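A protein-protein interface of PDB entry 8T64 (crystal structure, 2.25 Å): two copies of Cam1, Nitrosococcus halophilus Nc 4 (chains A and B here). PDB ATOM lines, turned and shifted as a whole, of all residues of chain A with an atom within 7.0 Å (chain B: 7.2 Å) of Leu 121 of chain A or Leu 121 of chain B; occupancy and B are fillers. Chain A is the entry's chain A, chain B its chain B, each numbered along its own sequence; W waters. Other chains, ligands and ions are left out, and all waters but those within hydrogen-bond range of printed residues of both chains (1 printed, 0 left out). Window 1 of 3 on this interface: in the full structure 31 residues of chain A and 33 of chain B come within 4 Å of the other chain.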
ATOM      1  N   THR A  33     -26.202 -23.584 -14.019  1.00  0.00           N
ATOM      2  CA  THR A  33     -25.414 -23.202 -15.171  1.00  0.00           C
ATOM      3  C   THR A  33     -24.061 -22.955 -14.527  1.00  0.00           C
ATOM      4  O   THR A  33     -23.964 -22.310 -13.540  1.00  0.00           O
ATOM      5  CB  THR A  33     -25.907 -21.967 -15.903  1.00  0.00           C
ATOM      6  OG1 THR A  33     -26.327 -20.999 -14.972  1.00  0.00           O
ATOM      7  CG2 THR A  33     -27.026 -22.313 -16.751  1.00  0.00           C
ATOM      8  N   PRO A  87     -21.773 -21.441 -26.367  1.00  0.00           N
ATOM      9  CA  PRO A  87     -22.225 -20.704 -25.184  1.00  0.00           C
ATOM     10  C   PRO A  87     -22.943 -19.401 -25.509  1.00  0.00           C
ATOM     11  O   PRO A  87     -23.629 -18.868 -24.623  1.00  0.00           O
ATOM     12  CB  PRO A  87     -20.923 -20.470 -24.402  1.00  0.00           C
ATOM     13  CG  PRO A  87     -19.823 -20.592 -25.394  1.00  0.00           C
ATOM     14  CD  PRO A  87     -20.303 -21.582 -26.418  1.00  0.00           C
ATOM     15  N   ASN A  88     -22.816 -18.869 -26.735  1.00  0.00           N
ATOM     16  CA  ASN A  88     -23.544 -17.668 -27.142  1.00  0.00           C
ATOM     17  C   ASN A  88     -24.920 -17.963 -27.720  1.00  0.00           C
ATOM     18  O   ASN A  88     -25.722 -17.042 -27.856  1.00  0.00           O
ATOM     19  CB  ASN A  88     -22.745 -16.864 -28.170  1.00  0.00           C
ATOM     20  CG  ASN A  88     -21.429 -16.360 -27.611  1.00  0.00           C
ATOM     21  OD1 ASN A  88     -21.395 -15.517 -26.706  1.00  0.00           O
ATOM     22  ND2 ASN A  88     -20.335 -16.899 -28.127  1.00  0.00           N
ATOM     23  N   PRO A  90     -28.422 -19.097 -26.994  1.00  0.00           N
ATOM     24  CA  PRO A  90     -29.282 -19.440 -25.850  1.00  0.00           C
ATOM     25  C   PRO A  90     -30.159 -20.656 -26.085  1.00  0.00           C
ATOM     26  O   PRO A  90     -30.638 -21.247 -25.107  1.00  0.00           O
ATOM     27  CB  PRO A  90     -30.116 -18.171 -25.630  1.00  0.00           C
ATOM     28  CG  PRO A  90     -30.002 -17.396 -26.895  1.00  0.00           C
ATOM     29  CD  PRO A  90     -28.712 -17.756 -27.537  1.00  0.00           C
ATOM     30  N   ASP A 115     -30.756 -22.375 -10.758  1.00  0.00           N
ATOM     31  CA  ASP A 115     -29.818 -21.301 -10.441  1.00  0.00           C
ATOM     32  C   ASP A 115     -29.044 -20.952 -11.703  1.00  0.00           C
ATOM     33  O   ASP A 115     -28.290 -21.780 -12.227  1.00  0.00           O
ATOM     34  CB  ASP A 115     -28.853 -21.676  -9.317  1.00  0.00           C
ATOM     35  CG  ASP A 115     -27.742 -20.607  -9.096  1.00  0.00           C
ATOM     36  OD1 ASP A 115     -27.684 -19.578  -9.821  1.00  0.00           O
ATOM     37  OD2 ASP A 115     -26.929 -20.790  -8.156  1.00  0.00           O
ATOM     38  N   LEU A 116     -29.215 -19.717 -12.172  1.00  0.00           N
ATOM     39  CA  LEU A 116     -28.721 -19.303 -13.473  1.00  0.00           C
ATOM     40  C   LEU A 116     -27.615 -18.260 -13.378  1.00  0.00           C
ATOM     41  O   LEU A 116     -27.347 -17.568 -14.366  1.00  0.00           O
ATOM     42  CB  LEU A 116     -29.864 -18.779 -14.341  1.00  0.00           C
ATOM     43  CG  LEU A 116     -30.940 -17.872 -13.749  1.00  0.00           C
ATOM     44  CD1 LEU A 116     -30.344 -16.563 -13.270  1.00  0.00           C
ATOM     45  CD2 LEU A 116     -32.003 -17.630 -14.806  1.00  0.00           C
ATOM     46  N   THR A 117     -27.032 -18.079 -12.196  1.00  0.00           N
ATOM     47  CA  THR A 117     -25.740 -17.429 -12.111  1.00  0.00           C
ATOM     48  C   THR A 117     -24.746 -18.271 -12.907  1.00  0.00           C
ATOM     49  O   THR A 117     -25.002 -19.427 -13.238  1.00  0.00           O
ATOM     50  CB  THR A 117     -25.282 -17.316 -10.649  1.00  0.00           C
ATOM     51  OG1 THR A 117     -26.397 -17.066  -9.785  1.00  0.00           O
ATOM     52  CG2 THR A 117     -24.238 -16.214 -10.471  1.00  0.00           C
ATOM     53  N   GLY A 118     -23.575 -17.792 -13.236  1.00  0.00           N
ATOM     54  CA  GLY A 118     -22.631 -18.680 -13.921  1.00  0.00           C
ATOM     55  C   GLY A 118     -22.823 -18.888 -15.392  1.00  0.00           C
ATOM     56  O   GLY A 118     -23.845 -19.203 -15.958  1.00  0.00           O
ATOM     57  N   GLY A 119     -21.746 -18.592 -16.067  1.00  0.00           N
ATOM     58  CA  GLY A 119     -21.749 -18.625 -17.487  1.00  0.00           C
ATOM     59  C   GLY A 119     -22.088 -17.257 -17.978  1.00  0.00           C
ATOM     60  O   GLY A 119     -22.460 -16.358 -17.281  1.00  0.00           O
ATOM     61  N   LYS A 120     -22.000 -17.106 -19.269  1.00  0.00           N
ATOM     62  CA  LYS A 120     -22.321 -15.850 -19.900  1.00  0.00           C
ATOM     63  C   LYS A 120     -23.803 -15.618 -19.956  1.00  0.00           C
ATOM     64  O   LYS A 120     -24.592 -16.498 -19.774  1.00  0.00           O
ATOM     65  CB  LYS A 120     -21.855 -15.898 -21.340  1.00  0.00           C
ATOM     66  CG  LYS A 120     -20.379 -15.853 -21.563  1.00  0.00           C
ATOM     67  CD  LYS A 120     -20.051 -16.265 -22.973  1.00  0.00           C
ATOM     68  CE  LYS A 120     -19.477 -15.111 -23.776  1.00  0.00           C
ATOM     69  NZ  LYS A 120     -18.133 -14.626 -23.340  1.00  0.00           N
ATOM     70  N   LEU A 121     -24.168 -14.420 -20.311  1.00  0.00           N
ATOM     71  CA  LEU A 121     -25.561 -14.032 -20.456  1.00  0.00           C
ATOM     72  C   LEU A 121     -26.447 -14.998 -21.255  1.00  0.00           C
ATOM     73  O   LEU A 121     -27.451 -15.412 -20.765  1.00  0.00           O
ATOM     74  CB  LEU A 121     -25.635 -12.654 -21.061  1.00  0.00           C
ATOM     75  CG  LEU A 121     -26.932 -11.881 -20.981  1.00  0.00           C
ATOM     76  CD1 LEU A 121     -27.653 -12.208 -19.705  1.00  0.00           C
ATOM     77  CD2 LEU A 121     -26.623 -10.397 -20.994  1.00  0.00           C
ATOM     78  N   PRO A 122     -26.040 -15.370 -22.478  1.00  0.00           N
ATOM     79  CA  PRO A 122     -26.789 -16.303 -23.312  1.00  0.00           C
ATOM     80  C   PRO A 122     -27.078 -17.565 -22.572  1.00  0.00           C
ATOM     81  O   PRO A 122     -28.132 -18.057 -22.696  1.00  0.00           O
ATOM     82  CB  PRO A 122     -25.842 -16.582 -24.458  1.00  0.00           C
ATOM     83  CG  PRO A 122     -25.071 -15.357 -24.575  1.00  0.00           C
ATOM     84  CD  PRO A 122     -24.900 -14.815 -23.204  1.00  0.00           C
ATOM     85  N   MET A 123     -26.123 -18.096 -21.856  1.00  0.00           N
ATOM     86  CA  MET A 123     -26.368 -19.286 -21.045  1.00  0.00           C
ATOM     87  C   MET A 123     -27.454 -19.036 -20.009  1.00  0.00           C
ATOM     88  O   MET A 123     -28.414 -19.808 -19.899  1.00  0.00           O
ATOM     89  CB  MET A 123     -25.075 -19.724 -20.339  1.00  0.00           C
ATOM     90  CG  MET A 123     -24.200 -20.730 -21.074  1.00  0.00           C
ATOM     91  SD  MET A 123     -23.560 -21.940 -19.849  1.00  0.00           S
ATOM     92  CE  MET A 123     -24.991 -22.958 -19.636  1.00  0.00           C
ATOM     93  N   SER A 124     -27.287 -17.987 -19.199  1.00  0.00           N
ATOM     94  CA  SER A 124     -28.279 -17.665 -18.170  1.00  0.00           C
ATOM     95  C   SER A 124     -29.669 -17.489 -18.769  1.00  0.00           C
ATOM     96  O   SER A 124     -30.658 -17.952 -18.189  1.00  0.00           O
ATOM     97  CB  SER A 124     -27.868 -16.393 -17.425  1.00  0.00           C
ATOM     98  OG  SER A 124     -26.636 -16.575 -16.741  1.00  0.00           O
ATOM     99  N   LEU A 125     -29.759 -16.809 -19.931  1.00  0.00           N
ATOM    100  CA  LEU A 125     -31.047 -16.522 -20.562  1.00  0.00           C
ATOM    101  C   LEU A 125     -31.665 -17.776 -21.142  1.00  0.00           C
ATOM    102  O   LEU A 125     -32.880 -17.954 -21.078  1.00  0.00           O
ATOM    103  CB  LEU A 125     -30.890 -15.487 -21.685  1.00  0.00           C
ATOM    104  CG  LEU A 125     -30.568 -14.033 -21.360  1.00  0.00           C
ATOM    105  CD1 LEU A 125     -30.529 -13.205 -22.625  1.00  0.00           C
ATOM    106  CD2 LEU A 125     -31.631 -13.498 -20.479  1.00  0.00           C
ATOM    107  N   GLY A 126     -30.844 -18.628 -21.763  1.00  0.00           N
ATOM    108  CA  GLY A 126     -31.329 -19.939 -22.157  1.00  0.00           C
ATOM    109  C   GLY A 126     -31.889 -20.712 -20.974  1.00  0.00           C
ATOM    110  O   GLY A 126     -32.968 -21.300 -21.056  1.00  0.00           O
ATOM    111  N   ALA A 127     -31.169 -20.693 -19.846  1.00  0.00           N
ATOM    112  CA  ALA A 127     -31.653 -21.360 -18.641  1.00  0.00           C
ATOM    113  C   ALA A 127     -32.931 -20.716 -18.133  1.00  0.00           C
ATOM    114  O   ALA A 127     -33.827 -21.415 -17.648  1.00  0.00           O
ATOM    115  CB  ALA A 127     -30.587 -21.342 -17.544  1.00  0.00           C
ATOM    116  N   LEU A 139     -33.371 -18.805  -9.845  1.00  0.00           N
ATOM    117  CA  LEU A 139     -32.666 -18.144  -8.759  1.00  0.00           C
ATOM    118  C   LEU A 139     -31.417 -17.460  -9.286  1.00  0.00           C
ATOM    119  O   LEU A 139     -30.941 -17.750 -10.382  1.00  0.00           O
ATOM    120  CB  LEU A 139     -32.257 -19.124  -7.659  1.00  0.00           C
ATOM    121  CG  LEU A 139     -33.385 -19.934  -7.027  1.00  0.00           C
ATOM    122  CD1 LEU A 139     -32.838 -20.977  -6.070  1.00  0.00           C
ATOM    123  CD2 LEU A 139     -34.312 -18.991  -6.308  1.00  0.00           C
ATOM    124  N   TYR A 140     -30.866 -16.579  -8.464  1.00  0.00           N
ATOM    125  CA  TYR A 140     -29.679 -15.829  -8.816  1.00  0.00           C
ATOM    126  C   TYR A 140     -28.965 -15.459  -7.528  1.00  0.00           C
ATOM    127  O   TYR A 140     -29.615 -15.130  -6.535  1.00  0.00           O
ATOM    128  CB  TYR A 140     -30.053 -14.574  -9.616  1.00  0.00           C
ATOM    129  CG  TYR A 140     -28.933 -13.570  -9.737  1.00  0.00           C
ATOM    130  CD1 TYR A 140     -27.821 -13.847 -10.513  1.00  0.00           C
ATOM    131  CD2 TYR A 140     -28.993 -12.346  -9.079  1.00  0.00           C
ATOM    132  CE1 TYR A 140     -26.781 -12.932 -10.642  1.00  0.00           C
ATOM    133  CE2 TYR A 140     -27.970 -11.421  -9.196  1.00  0.00           C
ATOM    134  CZ  TYR A 140     -26.856 -11.715  -9.985  1.00  0.00           C
ATOM    135  OH  TYR A 140     -25.818 -10.801 -10.122  1.00  0.00           O
ATOM    136  N   VAL A 141     -27.638 -15.513  -7.546  1.00  0.00           N
ATOM    137  CA  VAL A 141     -26.820 -15.139  -6.399  1.00  0.00           C
ATOM    138  C   VAL A 141     -26.323 -13.714  -6.612  1.00  0.00           C
ATOM    139  O   VAL A 141     -25.478 -13.469  -7.475  1.00  0.00           O
ATOM    140  CB  VAL A 141     -25.643 -16.103  -6.205  1.00  0.00           C
ATOM    141  CG1 VAL A 141     -24.771 -15.639  -5.062  1.00  0.00           C
ATOM    142  CG2 VAL A 141     -26.158 -17.499  -5.966  1.00  0.00           C
ATOM    143  N   ILE A 162     -31.563 -12.794 -29.977  1.00  0.00           N
ATOM    144  CA  ILE A 162     -31.795 -13.834 -29.017  1.00  0.00           C
ATOM    145  C   ILE A 162     -33.230 -14.272 -28.838  1.00  0.00           C
ATOM    146  O   ILE A 162     -33.489 -15.290 -28.269  1.00  0.00           O
ATOM    147  CB  ILE A 162     -31.222 -13.363 -27.690  1.00  0.00           C
ATOM    148  CG1 ILE A 162     -29.805 -13.850 -27.564  1.00  0.00           C
ATOM    149  CG2 ILE A 162     -32.045 -13.821 -26.522  1.00  0.00           C
ATOM    150  CD1 ILE A 162     -29.133 -13.359 -26.320  1.00  0.00           C
ATOM    151  N   THR B  33     -29.812  -1.641 -21.725  1.00  0.00           N
ATOM    152  CA  THR B  33     -29.359  -1.702 -20.339  1.00  0.00           C
ATOM    153  C   THR B  33     -27.857  -1.442 -20.323  1.00  0.00           C
ATOM    154  O   THR B  33     -27.125  -1.931 -21.185  1.00  0.00           O
ATOM    155  CB  THR B  33     -29.686  -3.057 -19.684  1.00  0.00           C
ATOM    156  OG1 THR B  33     -29.223  -4.136 -20.502  1.00  0.00           O
ATOM    157  CG2 THR B  33     -31.170  -3.205 -19.476  1.00  0.00           C
ATOM    158  N   PRO B  87     -30.906  -2.762  -8.492  1.00  0.00           N
ATOM    159  CA  PRO B  87     -30.531  -3.555  -9.676  1.00  0.00           C
ATOM    160  C   PRO B  87     -30.630  -5.064  -9.494  1.00  0.00           C
ATOM    161  O   PRO B  87     -30.721  -5.773 -10.503  1.00  0.00           O
ATOM    162  CB  PRO B  87     -29.081  -3.135  -9.925  1.00  0.00           C
ATOM    163  CG  PRO B  87     -28.603  -2.671  -8.583  1.00  0.00           C
ATOM    164  CD  PRO B  87     -29.771  -1.984  -7.969  1.00  0.00           C
ATOM    165  N   ASN B  88     -30.594  -5.587  -8.270  1.00  0.00           N
ATOM    166  CA  ASN B  88     -30.769  -7.019  -8.068  1.00  0.00           C
ATOM    167  C   ASN B  88     -32.221  -7.480  -8.194  1.00  0.00           C
ATOM    168  O   ASN B  88     -32.470  -8.691  -8.142  1.00  0.00           O
ATOM    169  CB  ASN B  88     -30.215  -7.412  -6.705  1.00  0.00           C
ATOM    170  CG  ASN B  88     -28.718  -7.267  -6.639  1.00  0.00           C
ATOM    171  OD1 ASN B  88     -27.990  -7.769  -7.507  1.00  0.00           O
ATOM    172  ND2 ASN B  88     -28.241  -6.567  -5.614  1.00  0.00           N
ATOM    173  N   PRO B  90     -35.102  -7.943 -10.746  1.00  0.00           N
ATOM    174  CA  PRO B  90     -35.477  -7.877 -12.173  1.00  0.00           C
ATOM    175  C   PRO B  90     -36.719  -7.045 -12.467  1.00  0.00           C
ATOM    176  O   PRO B  90     -36.794  -6.429 -13.541  1.00  0.00           O
ATOM    177  CB  PRO B  90     -35.682  -9.353 -12.552  1.00  0.00           C
ATOM    178  CG  PRO B  90     -35.665 -10.127 -11.239  1.00  0.00           C
ATOM    179  CD  PRO B  90     -34.823  -9.320 -10.311  1.00  0.00           C
ATOM    180  N   ASP B 115     -31.168  -4.306 -26.596  1.00  0.00           N
ATOM    181  CA  ASP B 115     -29.842  -4.884 -26.349  1.00  0.00           C
ATOM    182  C   ASP B 115     -29.636  -5.027 -24.843  1.00  0.00           C
ATOM    183  O   ASP B 115     -29.446  -4.032 -24.137  1.00  0.00           O
ATOM    184  CB  ASP B 115     -28.743  -4.021 -26.965  1.00  0.00           C
ATOM    185  CG  ASP B 115     -27.343  -4.579 -26.722  1.00  0.00           C
ATOM    186  OD1 ASP B 115     -27.193  -5.598 -25.994  1.00  0.00           O
ATOM    187  OD2 ASP B 115     -26.380  -3.989 -27.263  1.00  0.00           O
ATOM    188  N   LEU B 116     -29.644  -6.258 -24.348  1.00  0.00           N
ATOM    189  CA  LEU B 116     -29.545  -6.491 -22.916  1.00  0.00           C
ATOM    190  C   LEU B 116     -28.138  -6.889 -22.472  1.00  0.00           C
ATOM    191  O   LEU B 116     -27.982  -7.480 -21.397  1.00  0.00           O
ATOM    192  CB  LEU B 116     -30.570  -7.544 -22.493  1.00  0.00           C
ATOM    193  CG  LEU B 116     -30.683  -8.784 -23.389  1.00  0.00           C
ATOM    194  CD1 LEU B 116     -29.617  -9.778 -23.051  1.00  0.00           C
ATOM    195  CD2 LEU B 116     -32.052  -9.441 -23.271  1.00  0.00           C
ATOM    196  N   THR B 117     -27.109  -6.560 -23.260  1.00  0.00           N
ATOM    197  CA  THR B 117     -25.746  -6.941 -22.886  1.00  0.00           C
ATOM    198  C   THR B 117     -25.326  -6.320 -21.559  1.00  0.00           C
ATOM    199  O   THR B 117     -24.681  -6.978 -20.739  1.00  0.00           O
ATOM    200  CB  THR B 117     -24.753  -6.543 -23.984  1.00  0.00           C
ATOM    201  OG1 THR B 117     -25.275  -6.939 -25.250  1.00  0.00           O
ATOM    202  CG2 THR B 117     -23.435  -7.242 -23.761  1.00  0.00           C
ATOM    203  N   GLY B 118     -25.670  -5.067 -21.328  1.00  0.00           N
ATOM    204  CA  GLY B 118     -25.128  -4.379 -20.178  1.00  0.00           C
ATOM    205  C   GLY B 118     -25.913  -4.649 -18.906  1.00  0.00           C
ATOM    206  O   GLY B 118     -27.052  -5.131 -18.929  1.00  0.00           O
ATOM    207  N   GLY B 119     -25.284  -4.305 -17.778  1.00  0.00           N
ATOM    208  CA  GLY B 119     -25.903  -4.423 -16.475  1.00  0.00           C
ATOM    209  C   GLY B 119     -25.637  -5.764 -15.819  1.00  0.00           C
ATOM    210  O   GLY B 119     -25.099  -6.699 -16.413  1.00  0.00           O
ATOM    211  N   LYS B 120     -26.036  -5.860 -14.564  1.00  0.00           N
ATOM    212  CA  LYS B 120     -25.996  -7.165 -13.933  1.00  0.00           C
ATOM    213  C   LYS B 120     -27.066  -8.070 -14.520  1.00  0.00           C
ATOM    214  O   LYS B 120     -28.015  -7.628 -15.188  1.00  0.00           O
ATOM    215  CB  LYS B 120     -26.184  -7.059 -12.424  1.00  0.00           C
ATOM    216  CG  LYS B 120     -27.304  -6.138 -11.983  1.00  0.00           C
ATOM    217  CD  LYS B 120     -27.295  -6.076 -10.462  1.00  0.00           C
ATOM    218  CE  LYS B 120     -25.932  -5.613  -9.957  1.00  0.00           C
ATOM    219  NZ  LYS B 120     -26.005  -5.152  -8.553  1.00  0.00           N
ATOM    220  N   LEU B 121     -26.914  -9.359 -14.230  1.00  0.00           N
ATOM    221  CA  LEU B 121     -27.841 -10.371 -14.730  1.00  0.00           C
ATOM    222  C   LEU B 121     -29.316 -10.021 -14.532  1.00  0.00           C
ATOM    223  O   LEU B 121     -30.079 -10.157 -15.499  1.00  0.00           O
ATOM    224  CB  LEU B 121     -27.483 -11.728 -14.094  1.00  0.00           C
ATOM    225  CG  LEU B 121     -28.289 -12.948 -14.560  1.00  0.00           C
ATOM    226  CD1 LEU B 121     -28.500 -12.931 -16.077  1.00  0.00           C
ATOM    227  CD2 LEU B 121     -27.592 -14.226 -14.160  1.00  0.00           C
ATOM    228  N   PRO B 122     -29.789  -9.583 -13.345  1.00  0.00           N
ATOM    229  CA  PRO B 122     -31.232  -9.294 -13.201  1.00  0.00           C
ATOM    230  C   PRO B 122     -31.716  -8.130 -14.052  1.00  0.00           C
ATOM    231  O   PRO B 122     -32.907  -8.079 -14.407  1.00  0.00           O
ATOM    232  CB  PRO B 122     -31.383  -8.974 -11.706  1.00  0.00           C
ATOM    233  CG  PRO B 122     -30.163  -9.513 -11.053  1.00  0.00           C
ATOM    234  CD  PRO B 122     -29.075  -9.419 -12.065  1.00  0.00           C
ATOM    235  N   MET B 123     -30.841  -7.163 -14.338  1.00  0.00           N
ATOM    236  CA  MET B 123     -31.166  -6.113 -15.300  1.00  0.00           C
ATOM    237  C   MET B 123     -31.386  -6.693 -16.690  1.00  0.00           C
ATOM    238  O   MET B 123     -32.392  -6.396 -17.349  1.00  0.00           O
ATOM    239  CB  MET B 123     -30.041  -5.079 -15.350  1.00  0.00           C
ATOM    240  CG  MET B 123     -29.964  -4.154 -14.154  1.00  0.00           C
ATOM    241  SD  MET B 123     -29.327  -2.504 -14.616  1.00  0.00           S
ATOM    242  CE  MET B 123     -29.817  -2.423 -16.288  1.00  0.00           C
ATOM    243  N   SER B 124     -30.414  -7.479 -17.173  1.00  0.00           N
ATOM    244  CA  SER B 124     -30.578  -8.141 -18.460  1.00  0.00           C
ATOM    245  C   SER B 124     -31.823  -9.009 -18.454  1.00  0.00           C
ATOM    246  O   SER B 124     -32.551  -9.060 -19.448  1.00  0.00           O
ATOM    247  CB  SER B 124     -29.349  -8.990 -18.804  1.00  0.00           C
ATOM    248  OG  SER B 124     -28.142  -8.266 -18.732  1.00  0.00           O
ATOM    249  N   LEU B 125     -32.097  -9.683 -17.333  1.00  0.00           N
ATOM    250  CA  LEU B 125     -33.269 -10.547 -17.261  1.00  0.00           C
ATOM    251  C   LEU B 125     -34.558  -9.731 -17.263  1.00  0.00           C
ATOM    252  O   LEU B 125     -35.497 -10.053 -17.995  1.00  0.00           O
ATOM    253  CB  LEU B 125     -33.184 -11.444 -16.020  1.00  0.00           C
ATOM    254  CG  LEU B 125     -32.153 -12.569 -16.179  1.00  0.00           C
ATOM    255  CD1 LEU B 125     -32.005 -13.468 -14.954  1.00  0.00           C
ATOM    256  CD2 LEU B 125     -32.576 -13.396 -17.342  1.00  0.00           C
ATOM    257  N   GLY B 126     -34.620  -8.672 -16.457  1.00  0.00           N
ATOM    258  CA  GLY B 126     -35.774  -7.790 -16.506  1.00  0.00           C
ATOM    259  C   GLY B 126     -35.990  -7.179 -17.881  1.00  0.00           C
ATOM    260  O   GLY B 126     -37.126  -7.057 -18.342  1.00  0.00           O
ATOM    261  N   ALA B 127     -34.901  -6.800 -18.560  1.00  0.00           N
ATOM    262  CA  ALA B 127     -35.025  -6.222 -19.895  1.00  0.00           C
ATOM    263  C   ALA B 127     -35.584  -7.235 -20.884  1.00  0.00           C
ATOM    264  O   ALA B 127     -36.422  -6.896 -21.730  1.00  0.00           O
ATOM    265  CB  ALA B 127     -33.668  -5.711 -20.377  1.00  0.00           C
ATOM    266  N   LEU B 139     -31.376  -8.435 -28.295  1.00  0.00           N
ATOM    267  CA  LEU B 139     -30.063  -8.589 -28.899  1.00  0.00           C
ATOM    268  C   LEU B 139     -28.987  -8.763 -27.831  1.00  0.00           C
ATOM    269  O   LEU B 139     -29.151  -8.400 -26.664  1.00  0.00           O
ATOM    270  CB  LEU B 139     -29.723  -7.398 -29.804  1.00  0.00           C
ATOM    271  CG  LEU B 139     -30.882  -6.844 -30.645  1.00  0.00           C
ATOM    272  CD1 LEU B 139     -30.534  -5.472 -31.174  1.00  0.00           C
ATOM    273  CD2 LEU B 139     -31.252  -7.786 -31.792  1.00  0.00           C
ATOM    274  N   TYR B 140     -27.864  -9.323 -28.257  1.00  0.00           N
ATOM    275  CA  TYR B 140     -26.740  -9.542 -27.368  1.00  0.00           C
ATOM    276  C   TYR B 140     -25.475  -9.384 -28.181  1.00  0.00           C
ATOM    277  O   TYR B 140     -25.444  -9.692 -29.378  1.00  0.00           O
ATOM    278  CB  TYR B 140     -26.783 -10.930 -26.708  1.00  0.00           C
ATOM    279  CG  TYR B 140     -25.535 -11.307 -25.934  1.00  0.00           C
ATOM    280  CD1 TYR B 140     -25.283 -10.770 -24.674  1.00  0.00           C
ATOM    281  CD2 TYR B 140     -24.618 -12.210 -26.457  1.00  0.00           C
ATOM    282  CE1 TYR B 140     -24.159 -11.113 -23.960  1.00  0.00           C
ATOM    283  CE2 TYR B 140     -23.485 -12.560 -25.749  1.00  0.00           C
ATOM    284  CZ  TYR B 140     -23.261 -12.011 -24.498  1.00  0.00           C
ATOM    285  OH  TYR B 140     -22.141 -12.350 -23.786  1.00  0.00           O
ATOM    286  N   VAL B 141     -24.444  -8.893 -27.523  1.00  0.00           N
ATOM    287  CA  VAL B 141     -23.159  -8.644 -28.140  1.00  0.00           C
ATOM    288  C   VAL B 141     -22.202  -9.691 -27.588  1.00  0.00           C
ATOM    289  O   VAL B 141     -21.675  -9.549 -26.482  1.00  0.00           O
ATOM    290  CB  VAL B 141     -22.682  -7.222 -27.860  1.00  0.00           C
ATOM    291  CG1 VAL B 141     -21.362  -6.959 -28.562  1.00  0.00           C
ATOM    292  CG2 VAL B 141     -23.766  -6.246 -28.308  1.00  0.00           C
ATOM    293  N   ILE B 162     -35.749 -14.870  -9.064  1.00  0.00           N
ATOM    294  CA  ILE B 162     -35.888 -14.129 -10.293  1.00  0.00           C
ATOM    295  C   ILE B 162     -37.261 -14.325 -10.831  1.00  0.00           C
ATOM    296  O   ILE B 162     -37.865 -13.399 -11.288  1.00  0.00           O
ATOM    297  CB  ILE B 162     -34.971 -14.719 -11.372  1.00  0.00           C
ATOM    298  CG1 ILE B 162     -33.515 -14.407 -11.086  1.00  0.00           C
ATOM    299  CG2 ILE B 162     -35.383 -14.243 -12.746  1.00  0.00           C
ATOM    300  CD1 ILE B 162     -33.001 -13.189 -11.792  1.00  0.00           C
HETATM  301  O   HOH W   1     -22.363 -12.208 -20.555  1.00  0.00           O
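The side-chain hydroxyl (OG) of Ser 124 of chain B lies within hydrogen-bond range of the backbone carbonyl oxygen (O) of Leu 116 of chain B.
The side-chain hydroxyl (OG) of Ser 124 of chain B lies within hydrogen-bond range of the backbone carbonyl oxygen (O) of Gly 118 of chain B (3.3 Å).
The backbone NH (N) of Leu 116 of chain A lies within hydrogen-bond range of the backbone carbonyl oxygen (O) of Leu 139 of chain A (3.2 Å).
N of Val 141 of chain B lies within hydrogen-bond range of OG1 of Thr 117 of chain B (3.1 Å).
The backbone NH (N) of Leu 116 of chain B is in hydrogen-bond range of the backbone carbonyl oxygen (O) of Leu 139 of chain B (3.2 Å).
OD1 of Asp 115 of chain B is in hydrogen-bond range of OG1 of Thr 117 of chain B (2.5 Å).
Leu 116 of chain A touches Leu 125 of chain B (CD1 to CD1, 3.9 Å).
Tyr 140 of chain B touches Lys 120 of chain A.
Leu 121 of chain A touches Thr 117 of chain B (CD2 to O, 3.9 Å).
Leu 121 of chain A touches Ser 124 of chain B.
Leu 121 of chain A touches Tyr 140 of chain B (CB to CE1, 3.6 Å).
Pro 122 of chain A touches Tyr 140 of chain B (CG to CE2, 3.4 Å).
Ser 124 of chain A touches Leu 121 of chain B (OG to CD2, 3.6 Å).
Leu 125 of chain A touches Leu 116 of chain B (CD1 to CD1, 3.6 Å).
CD1 of Tyr 140 of chain A touches CD2 of Leu 121 of chain B, 3.7 Å away.
CE2 of Tyr 140 of chain A touches CG of Pro 122 of chain B, at 3.4 Å.
Printed residues of chain B within 4 Å of Asn 88 of chain A: Tyr 140 (3.7 Å).
Leu 121 of chain A touches just these residues of chain B: Leu 116, Thr 117, Leu 121, Ser 124 and Tyr 140.
Printed residues of chain A within 4 Å of Thr 117 of chain B: Leu 121.
Lys 120 of chain B touches none of the printed residues of chain A.
Of chain A, only Leu 116 (3.4 Å), Leu 121 (3.8 Å), Ser 124 (3.6 Å) and Tyr 140 (3.7 Å) come within 4 Å of Leu 121 of chain B.
Of the printed residues of chain A, Leu 125 of chain B touches Leu 116 and Leu 125.
The nearest residue of chain A that does not touch Leu 121 of chain B is Thr 117 of chain A (4.2 Å).
Of the 21 printed residues of chain A, 9 touch a printed residue of chain B.
Printed residues of chain A that touch a printed residue of chain B: Asn 88, Leu 116, Lys 120, Leu 121, Pro 122, Ser 124, Leu 125, Tyr 140 and Ile 162.
Hydrophobic or aromatic side chains of chain A within 4 Å of the printed part of chain B: Leu 116, Leu 121, Pro 122, Leu 125, Tyr 140 and Ile 162.
Of the 21 printed residues of chain B, 8 touch a printed residue of chain A.
Among the printed residues, 17 pairs touch across the chains.
Among the printed residues, no Asp or Glu carboxylate lies within 4 Å of a Lys or Arg side-chain nitrogen of the other chain.
Leu 116 of chain A touches Leu 121 of chain B, and with the chains exchanged Leu 121 of chain A touches Leu 116 of chain B.
Leu 121 of chain A touches Thr 117 of chain B, but with the chains exchanged Thr 117 of chain A does not touch Leu 121 of chain B (4.2 Å).
Leu 121 of chain A touches Tyr 140 of chain B, and with the chains exchanged Tyr 140 of chain A touches Leu 121 of chain B.
Tyr 140 of chain A touches Ile 162 of chain B, and with the chains exchanged Ile 162 of chain A touches Tyr 140 of chain B.
Of the 17 pairs that touch across the chains among the printed residues, 14 have their exchanged pair printed and touching as well.
Water W1 bridges the backbone NH (N) of Leu 121 of chain A (2.9 Å) and the side-chain hydroxyl (OH) of Tyr 140 of chain B (3.2 Å).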
